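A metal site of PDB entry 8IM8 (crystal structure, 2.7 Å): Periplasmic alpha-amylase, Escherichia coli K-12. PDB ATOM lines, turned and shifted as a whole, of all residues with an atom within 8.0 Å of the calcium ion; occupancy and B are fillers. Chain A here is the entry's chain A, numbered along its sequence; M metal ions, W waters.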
ATOM      1  N   MET A 313      16.795   5.902   6.690  1.00  0.00           N
ATOM      2  CA  MET A 313      18.195   5.531   6.513  1.00  0.00           C
ATOM      3  C   MET A 313      18.437   4.033   6.364  1.00  0.00           C
ATOM      4  O   MET A 313      19.550   3.647   6.001  1.00  0.00           O
ATOM      5  CB  MET A 313      19.052   6.054   7.673  1.00  0.00           C
ATOM      6  CG  MET A 313      19.505   7.507   7.537  1.00  0.00           C
ATOM      7  SD  MET A 313      20.293   8.169   9.062  1.00  0.00           S
ATOM      8  CE  MET A 313      21.599   7.007   9.381  1.00  0.00           C
ATOM      9  N   ASN A 314      17.446   3.176   6.631  1.00  0.00           N
ATOM     10  CA  ASN A 314      17.718   1.744   6.535  1.00  0.00           C
ATOM     11  C   ASN A 314      17.985   1.334   5.096  1.00  0.00           C
ATOM     12  O   ASN A 314      18.866   0.519   4.826  1.00  0.00           O
ATOM     13  CB  ASN A 314      16.546   0.920   7.068  1.00  0.00           C
ATOM     14  CG  ASN A 314      16.953  -0.517   7.431  1.00  0.00           C
ATOM     15  OD1 ASN A 314      18.136  -0.821   7.800  1.00  0.00           O
ATOM     16  ND2 ASN A 314      16.019  -1.441   7.177  1.00  0.00           N
ATOM     17  N   HIS A 315      17.221   1.880   4.154  1.00  0.00           N
ATOM     18  CA  HIS A 315      17.191   1.325   2.804  1.00  0.00           C
ATOM     19  C   HIS A 315      17.200   2.427   1.747  1.00  0.00           C
ATOM     20  O   HIS A 315      16.964   3.596   2.018  1.00  0.00           O
ATOM     21  CB  HIS A 315      15.983   0.416   2.620  1.00  0.00           C
ATOM     22  CG  HIS A 315      14.688   1.095   2.900  1.00  0.00           C
ATOM     23  ND1 HIS A 315      14.109   1.108   4.157  1.00  0.00           N
ATOM     24  CD2 HIS A 315      13.883   1.859   2.107  1.00  0.00           C
ATOM     25  CE1 HIS A 315      12.985   1.810   4.117  1.00  0.00           C
ATOM     26  NE2 HIS A 315      12.831   2.278   2.882  1.00  0.00           N
ATOM     27  N   ARG A 383      23.872  -3.796   1.028  1.00  0.00           N
ATOM     28  CA  ARG A 383      23.767  -5.245   0.997  1.00  0.00           C
ATOM     29  C   ARG A 383      22.559  -5.636   0.151  1.00  0.00           C
ATOM     30  O   ARG A 383      21.507  -5.013   0.270  1.00  0.00           O
ATOM     31  CB  ARG A 383      23.561  -5.798   2.408  1.00  0.00           C
ATOM     32  CG  ARG A 383      24.815  -5.825   3.267  1.00  0.00           C
ATOM     33  CD  ARG A 383      24.512  -6.335   4.694  1.00  0.00           C
ATOM     34  NE  ARG A 383      23.824  -5.344   5.510  1.00  0.00           N
ATOM     35  CZ  ARG A 383      24.446  -4.427   6.256  1.00  0.00           C
ATOM     36  NH1 ARG A 383      25.771  -4.403   6.364  1.00  0.00           N
ATOM     37  NH2 ARG A 383      23.725  -3.524   6.927  1.00  0.00           N
ATOM     38  N   ASP A 395      19.729 -11.022  11.132  1.00  0.00           N
ATOM     39  CA  ASP A 395      19.262 -10.199  12.242  1.00  0.00           C
ATOM     40  C   ASP A 395      18.587  -8.925  11.740  1.00  0.00           C
ATOM     41  O   ASP A 395      18.642  -8.561  10.558  1.00  0.00           O
ATOM     42  CB  ASP A 395      20.405  -9.833  13.176  1.00  0.00           C
ATOM     43  CG  ASP A 395      21.525  -9.073  12.486  1.00  0.00           C
ATOM     44  OD1 ASP A 395      21.609  -9.157  11.236  1.00  0.00           O
ATOM     45  OD2 ASP A 395      22.279  -8.342  13.178  1.00  0.00           O
ATOM     46  N   ASP A 396      17.978  -8.190  12.685  1.00  0.00           N
ATOM     47  CA  ASP A 396      17.195  -6.999  12.357  1.00  0.00           C
ATOM     48  C   ASP A 396      18.030  -5.912  11.674  1.00  0.00           C
ATOM     49  O   ASP A 396      17.545  -5.238  10.758  1.00  0.00           O
ATOM     50  CB  ASP A 396      16.520  -6.459  13.630  1.00  0.00           C
ATOM     51  CG  ASP A 396      15.292  -7.292  14.060  1.00  0.00           C
ATOM     52  OD1 ASP A 396      14.610  -7.880  13.188  1.00  0.00           O
ATOM     53  OD2 ASP A 396      14.987  -7.333  15.279  1.00  0.00           O
ATOM     54  N   LEU A 397      19.277  -5.703  12.101  1.00  0.00           N
ATOM     55  CA  LEU A 397      20.023  -4.553  11.612  1.00  0.00           C
ATOM     56  C   LEU A 397      20.438  -4.728  10.150  1.00  0.00           C
ATOM     57  O   LEU A 397      20.273  -3.805   9.326  1.00  0.00           O
ATOM     58  CB  LEU A 397      21.259  -4.316  12.495  1.00  0.00           C
ATOM     59  CG  LEU A 397      21.016  -4.001  13.981  1.00  0.00           C
ATOM     60  CD1 LEU A 397      22.346  -3.788  14.723  1.00  0.00           C
ATOM     61  CD2 LEU A 397      20.078  -2.811  14.215  1.00  0.00           C
ATOM     62  N   THR A 398      20.956  -5.908   9.814  1.00  0.00           N
ATOM     63  CA  THR A 398      21.453  -6.202   8.476  1.00  0.00           C
ATOM     64  C   THR A 398      20.445  -6.938   7.583  1.00  0.00           C
ATOM     65  O   THR A 398      20.772  -7.188   6.414  1.00  0.00           O
ATOM     66  CB  THR A 398      22.767  -7.006   8.537  1.00  0.00           C
ATOM     67  OG1 THR A 398      22.573  -8.218   9.279  1.00  0.00           O
ATOM     68  CG2 THR A 398      23.888  -6.205   9.168  1.00  0.00           C
ATOM     69  N   MET A 399      19.258  -7.287   8.070  1.00  0.00           N
ATOM     70  CA  MET A 399      18.321  -7.911   7.138  1.00  0.00           C
ATOM     71  C   MET A 399      17.767  -6.892   6.133  1.00  0.00           C
ATOM     72  O   MET A 399      17.888  -5.669   6.297  1.00  0.00           O
ATOM     73  CB  MET A 399      17.157  -8.595   7.861  1.00  0.00           C
ATOM     74  CG  MET A 399      16.246  -7.697   8.694  1.00  0.00           C
ATOM     75  SD  MET A 399      14.717  -8.579   9.154  1.00  0.00           S
ATOM     76  CE  MET A 399      15.363  -9.854  10.236  1.00  0.00           C
ATOM     77  N   SER A 400      17.151  -7.439   5.084  1.00  0.00           N
ATOM     78  CA  SER A 400      16.503  -6.709   4.001  1.00  0.00           C
ATOM     79  C   SER A 400      14.999  -6.843   4.129  1.00  0.00           C
ATOM     80  O   SER A 400      14.467  -7.965   4.070  1.00  0.00           O
ATOM     81  CB  SER A 400      16.961  -7.272   2.644  1.00  0.00           C
ATOM     82  OG  SER A 400      16.263  -6.661   1.560  1.00  0.00           O
ATOM     83  N   LEU A 401      14.294  -5.708   4.268  1.00  0.00           N
ATOM     84  CA  LEU A 401      12.829  -5.703   4.339  1.00  0.00           C
ATOM     85  C   LEU A 401      12.265  -5.577   2.929  1.00  0.00           C
ATOM     86  O   LEU A 401      12.622  -4.654   2.179  1.00  0.00           O
ATOM     87  CB  LEU A 401      12.315  -4.548   5.212  1.00  0.00           C
ATOM     88  CG  LEU A 401      12.433  -4.632   6.747  1.00  0.00           C
ATOM     89  CD1 LEU A 401      11.669  -5.790   7.377  1.00  0.00           C
ATOM     90  CD2 LEU A 401      13.881  -4.709   7.149  1.00  0.00           C
ATOM     91  N   LEU A 404      14.169  -4.597  -0.118  1.00  0.00           N
ATOM     92  CA  LEU A 404      14.793  -3.295  -0.239  1.00  0.00           C
ATOM     93  C   LEU A 404      16.247  -3.418   0.195  1.00  0.00           C
ATOM     94  O   LEU A 404      16.539  -4.094   1.181  1.00  0.00           O
ATOM     95  CB  LEU A 404      14.086  -2.271   0.628  1.00  0.00           C
ATOM     96  CG  LEU A 404      12.641  -1.835   0.345  1.00  0.00           C
ATOM     97  CD1 LEU A 404      12.078  -1.094   1.540  1.00  0.00           C
ATOM     98  CD2 LEU A 404      12.558  -0.931  -0.908  1.00  0.00           C
ATOM     99  N   PRO A 405      17.130  -2.720  -0.521  1.00  0.00           N
ATOM    100  CA  PRO A 405      18.514  -2.911  -0.160  1.00  0.00           C
ATOM    101  C   PRO A 405      18.866  -2.219   1.134  1.00  0.00           C
ATOM    102  O   PRO A 405      18.519  -1.059   1.298  1.00  0.00           O
ATOM    103  CB  PRO A 405      19.248  -2.266  -1.340  1.00  0.00           C
ATOM    104  CG  PRO A 405      18.237  -2.063  -2.410  1.00  0.00           C
ATOM    105  CD  PRO A 405      16.998  -1.783  -1.642  1.00  0.00           C
ATOM    106  N   ASP A 406      19.563  -2.904   2.022  1.00  0.00           N
ATOM    107  CA  ASP A 406      19.949  -2.332   3.297  1.00  0.00           C
ATOM    108  C   ASP A 406      21.237  -1.574   3.224  1.00  0.00           C
ATOM    109  O   ASP A 406      22.260  -2.105   2.842  1.00  0.00           O
ATOM    110  CB  ASP A 406      20.080  -3.459   4.320  1.00  0.00           C
ATOM    111  CG  ASP A 406      20.538  -2.975   5.668  1.00  0.00           C
ATOM    112  OD1 ASP A 406      20.159  -1.862   6.082  1.00  0.00           O
ATOM    113  OD2 ASP A 406      21.263  -3.739   6.325  1.00  0.00           O
ATOM    114  N   ILE A 407      21.175  -0.317   3.618  1.00  0.00           N
ATOM    115  CA  ILE A 407      22.368   0.494   3.625  1.00  0.00           C
ATOM    116  C   ILE A 407      23.315   0.111   4.746  1.00  0.00           C
ATOM    117  O   ILE A 407      22.896  -0.182   5.845  1.00  0.00           O
ATOM    118  CB  ILE A 407      21.995   1.977   3.737  1.00  0.00           C
ATOM    119  CG1 ILE A 407      20.975   2.332   2.663  1.00  0.00           C
ATOM    120  CG2 ILE A 407      23.236   2.851   3.627  1.00  0.00           C
ATOM    121  CD1 ILE A 407      20.319   3.678   2.875  1.00  0.00           C
ATOM    122  N   LYS A 408      24.588   0.097   4.433  1.00  0.00           N
ATOM    123  CA  LYS A 408      25.652  -0.257   5.375  1.00  0.00           C
ATOM    124  C   LYS A 408      25.940   0.906   6.335  1.00  0.00           C
ATOM    125  O   LYS A 408      26.998   1.530   6.307  1.00  0.00           O
ATOM    126  CB  LYS A 408      26.914  -0.630   4.618  1.00  0.00           C
ATOM    127  CG  LYS A 408      26.886  -1.972   3.967  1.00  0.00           C
ATOM    128  CD  LYS A 408      28.208  -2.163   3.276  1.00  0.00           C
ATOM    129  CE  LYS A 408      28.356  -3.572   2.747  1.00  0.00           C
ATOM    130  NZ  LYS A 408      29.655  -3.705   2.055  1.00  0.00           N
ATOM    131  N   THR A 409      24.931   1.194   7.164  1.00  0.00           N
ATOM    132  CA  THR A 409      25.078   2.260   8.133  1.00  0.00           C
ATOM    133  C   THR A 409      26.231   2.001   9.099  1.00  0.00           C
ATOM    134  O   THR A 409      26.925   2.948   9.502  1.00  0.00           O
ATOM    135  CB  THR A 409      23.768   2.442   8.910  1.00  0.00           C
ATOM    136  OG1 THR A 409      23.378   1.191   9.479  1.00  0.00           O
ATOM    137  CG2 THR A 409      22.673   2.943   7.998  1.00  0.00           C
ATOM    138  N   GLU A 410      26.493   0.733   9.455  1.00  0.00           N
ATOM    139  CA  GLU A 410      27.565   0.420  10.406  1.00  0.00           C
ATOM    140  C   GLU A 410      28.971   0.501   9.781  1.00  0.00           C
ATOM    141  O   GLU A 410      29.950   0.583  10.521  1.00  0.00           O
ATOM    142  CB  GLU A 410      27.394  -0.985  10.965  1.00  0.00           C
ATOM    143  CG  GLU A 410      27.990  -1.982  10.017  1.00  0.00           C
ATOM    144  CD  GLU A 410      27.112  -2.225   8.778  1.00  0.00           C
ATOM    145  OE1 GLU A 410      25.996  -1.635   8.674  1.00  0.00           O
ATOM    146  OE2 GLU A 410      27.592  -2.928   7.864  1.00  0.00           O
ATOM    147  N   THR A 461      11.515   2.706  10.046  1.00  0.00           N
ATOM    148  CA  THR A 461      12.170   1.440  10.364  1.00  0.00           C
ATOM    149  C   THR A 461      13.278   1.438  11.396  1.00  0.00           C
ATOM    150  O   THR A 461      14.345   0.868  11.175  1.00  0.00           O
ATOM    151  CB  THR A 461      12.616   0.696   9.084  1.00  0.00           C
ATOM    152  OG1 THR A 461      13.183   1.604   8.124  1.00  0.00           O
ATOM    153  CG2 THR A 461      11.459  -0.033   8.438  1.00  0.00           C
ATOM    154  N   LYS A 463      13.987   0.082  14.175  1.00  0.00           N
ATOM    155  CA  LYS A 463      14.576  -1.154  14.684  1.00  0.00           C
ATOM    156  C   LYS A 463      15.706  -1.696  13.817  1.00  0.00           C
ATOM    157  O   LYS A 463      16.542  -2.461  14.328  1.00  0.00           O
ATOM    158  CB  LYS A 463      13.506  -2.253  14.851  1.00  0.00           C
ATOM    159  CG  LYS A 463      12.617  -2.013  16.065  1.00  0.00           C
ATOM    160  CD  LYS A 463      11.527  -3.065  16.442  1.00  0.00           C
ATOM    161  CE  LYS A 463      10.930  -2.587  17.850  1.00  0.00           C
ATOM    162  NZ  LYS A 463       9.788  -3.326  18.514  1.00  0.00           N
ATOM    163  N   HIS A 464      15.784  -1.323  12.543  1.00  0.00           N
ATOM    164  CA  HIS A 464      16.642  -1.996  11.570  1.00  0.00           C
ATOM    165  C   HIS A 464      17.935  -1.235  11.264  1.00  0.00           C
ATOM    166  O   HIS A 464      18.639  -1.578  10.308  1.00  0.00           O
ATOM    167  CB  HIS A 464      15.840  -2.258  10.302  1.00  0.00           C
ATOM    168  CG  HIS A 464      14.665  -3.166  10.539  1.00  0.00           C
ATOM    169  ND1 HIS A 464      14.789  -4.530  10.693  1.00  0.00           N
ATOM    170  CD2 HIS A 464      13.341  -2.888  10.694  1.00  0.00           C
ATOM    171  CE1 HIS A 464      13.597  -5.060  10.893  1.00  0.00           C
ATOM    172  NE2 HIS A 464      12.701  -4.085  10.897  1.00  0.00           N
ATOM    173  N   VAL A 465      18.253  -0.225  12.072  1.00  0.00           N
ATOM    174  CA  VAL A 465      19.511   0.499  12.030  1.00  0.00           C
ATOM    175  C   VAL A 465      20.047   0.621  13.452  1.00  0.00           C
ATOM    176  O   VAL A 465      19.272   0.832  14.391  1.00  0.00           O
ATOM    177  CB  VAL A 465      19.338   1.893  11.376  1.00  0.00           C
ATOM    178  CG1 VAL A 465      20.586   2.757  11.527  1.00  0.00           C
ATOM    179  CG2 VAL A 465      18.934   1.754   9.907  1.00  0.00           C
ATOM    180  N   GLU A 466      21.349   0.445  13.611  1.00  0.00           N
ATOM    181  CA  GLU A 466      21.974   0.486  14.928  1.00  0.00           C
ATOM    182  C   GLU A 466      21.821   1.862  15.584  1.00  0.00           C
ATOM    183  O   GLU A 466      21.886   2.896  14.920  1.00  0.00           O
ATOM    184  CB  GLU A 466      23.452   0.130  14.820  1.00  0.00           C
ATOM    185  CG  GLU A 466      24.269   1.195  14.085  1.00  0.00           C
ATOM    186  CD  GLU A 466      24.175   1.102  12.540  1.00  0.00           C
ATOM    187  OE1 GLU A 466      23.234   0.453  12.024  1.00  0.00           O
ATOM    188  OE2 GLU A 466      25.059   1.667  11.843  1.00  0.00           O
HETATM  189 CA    CA M   1      19.287  -2.451   8.105  1.00  0.00          CA
HETATM  190  O   HOH W   1      20.848  -1.145   8.529  1.00  0.00           O
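The calcium ion is bound by OD1 of Asn 314 (2.0 Å), O of Leu 397 (2.1 Å), water W1 (2.1 Å), OD1 of Asp 406 (2.3 Å) and O of His 464 (2.5 Å). Slightly farther from the calcium ion lies OD2 of Asp 406 (3.0 Å).
O of Asn 314 lies within hydrogen-bond range of N of Ile 407, at 2.7 Å. The side-chain carboxylate (OD2) of Asp 406 lies within salt-bridge range of the guanidinium group (NH2) of Arg 383 (2.5 Å). A ring nitrogen (ND1) of His 464 sits at hydrogen-bond distance from the backbone carbonyl oxygen (O) of Asp 396, at 2.8 Å.
Residues that only touch the calcium ion: Met 399 (3.9 Å). Within 4 Å of the calcium ion: Asn 314, Leu 397, Met 399, Asp 406 and His 464. The nearest printed residue that does not touch the calcium ion is Thr 398 (4.2 Å).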
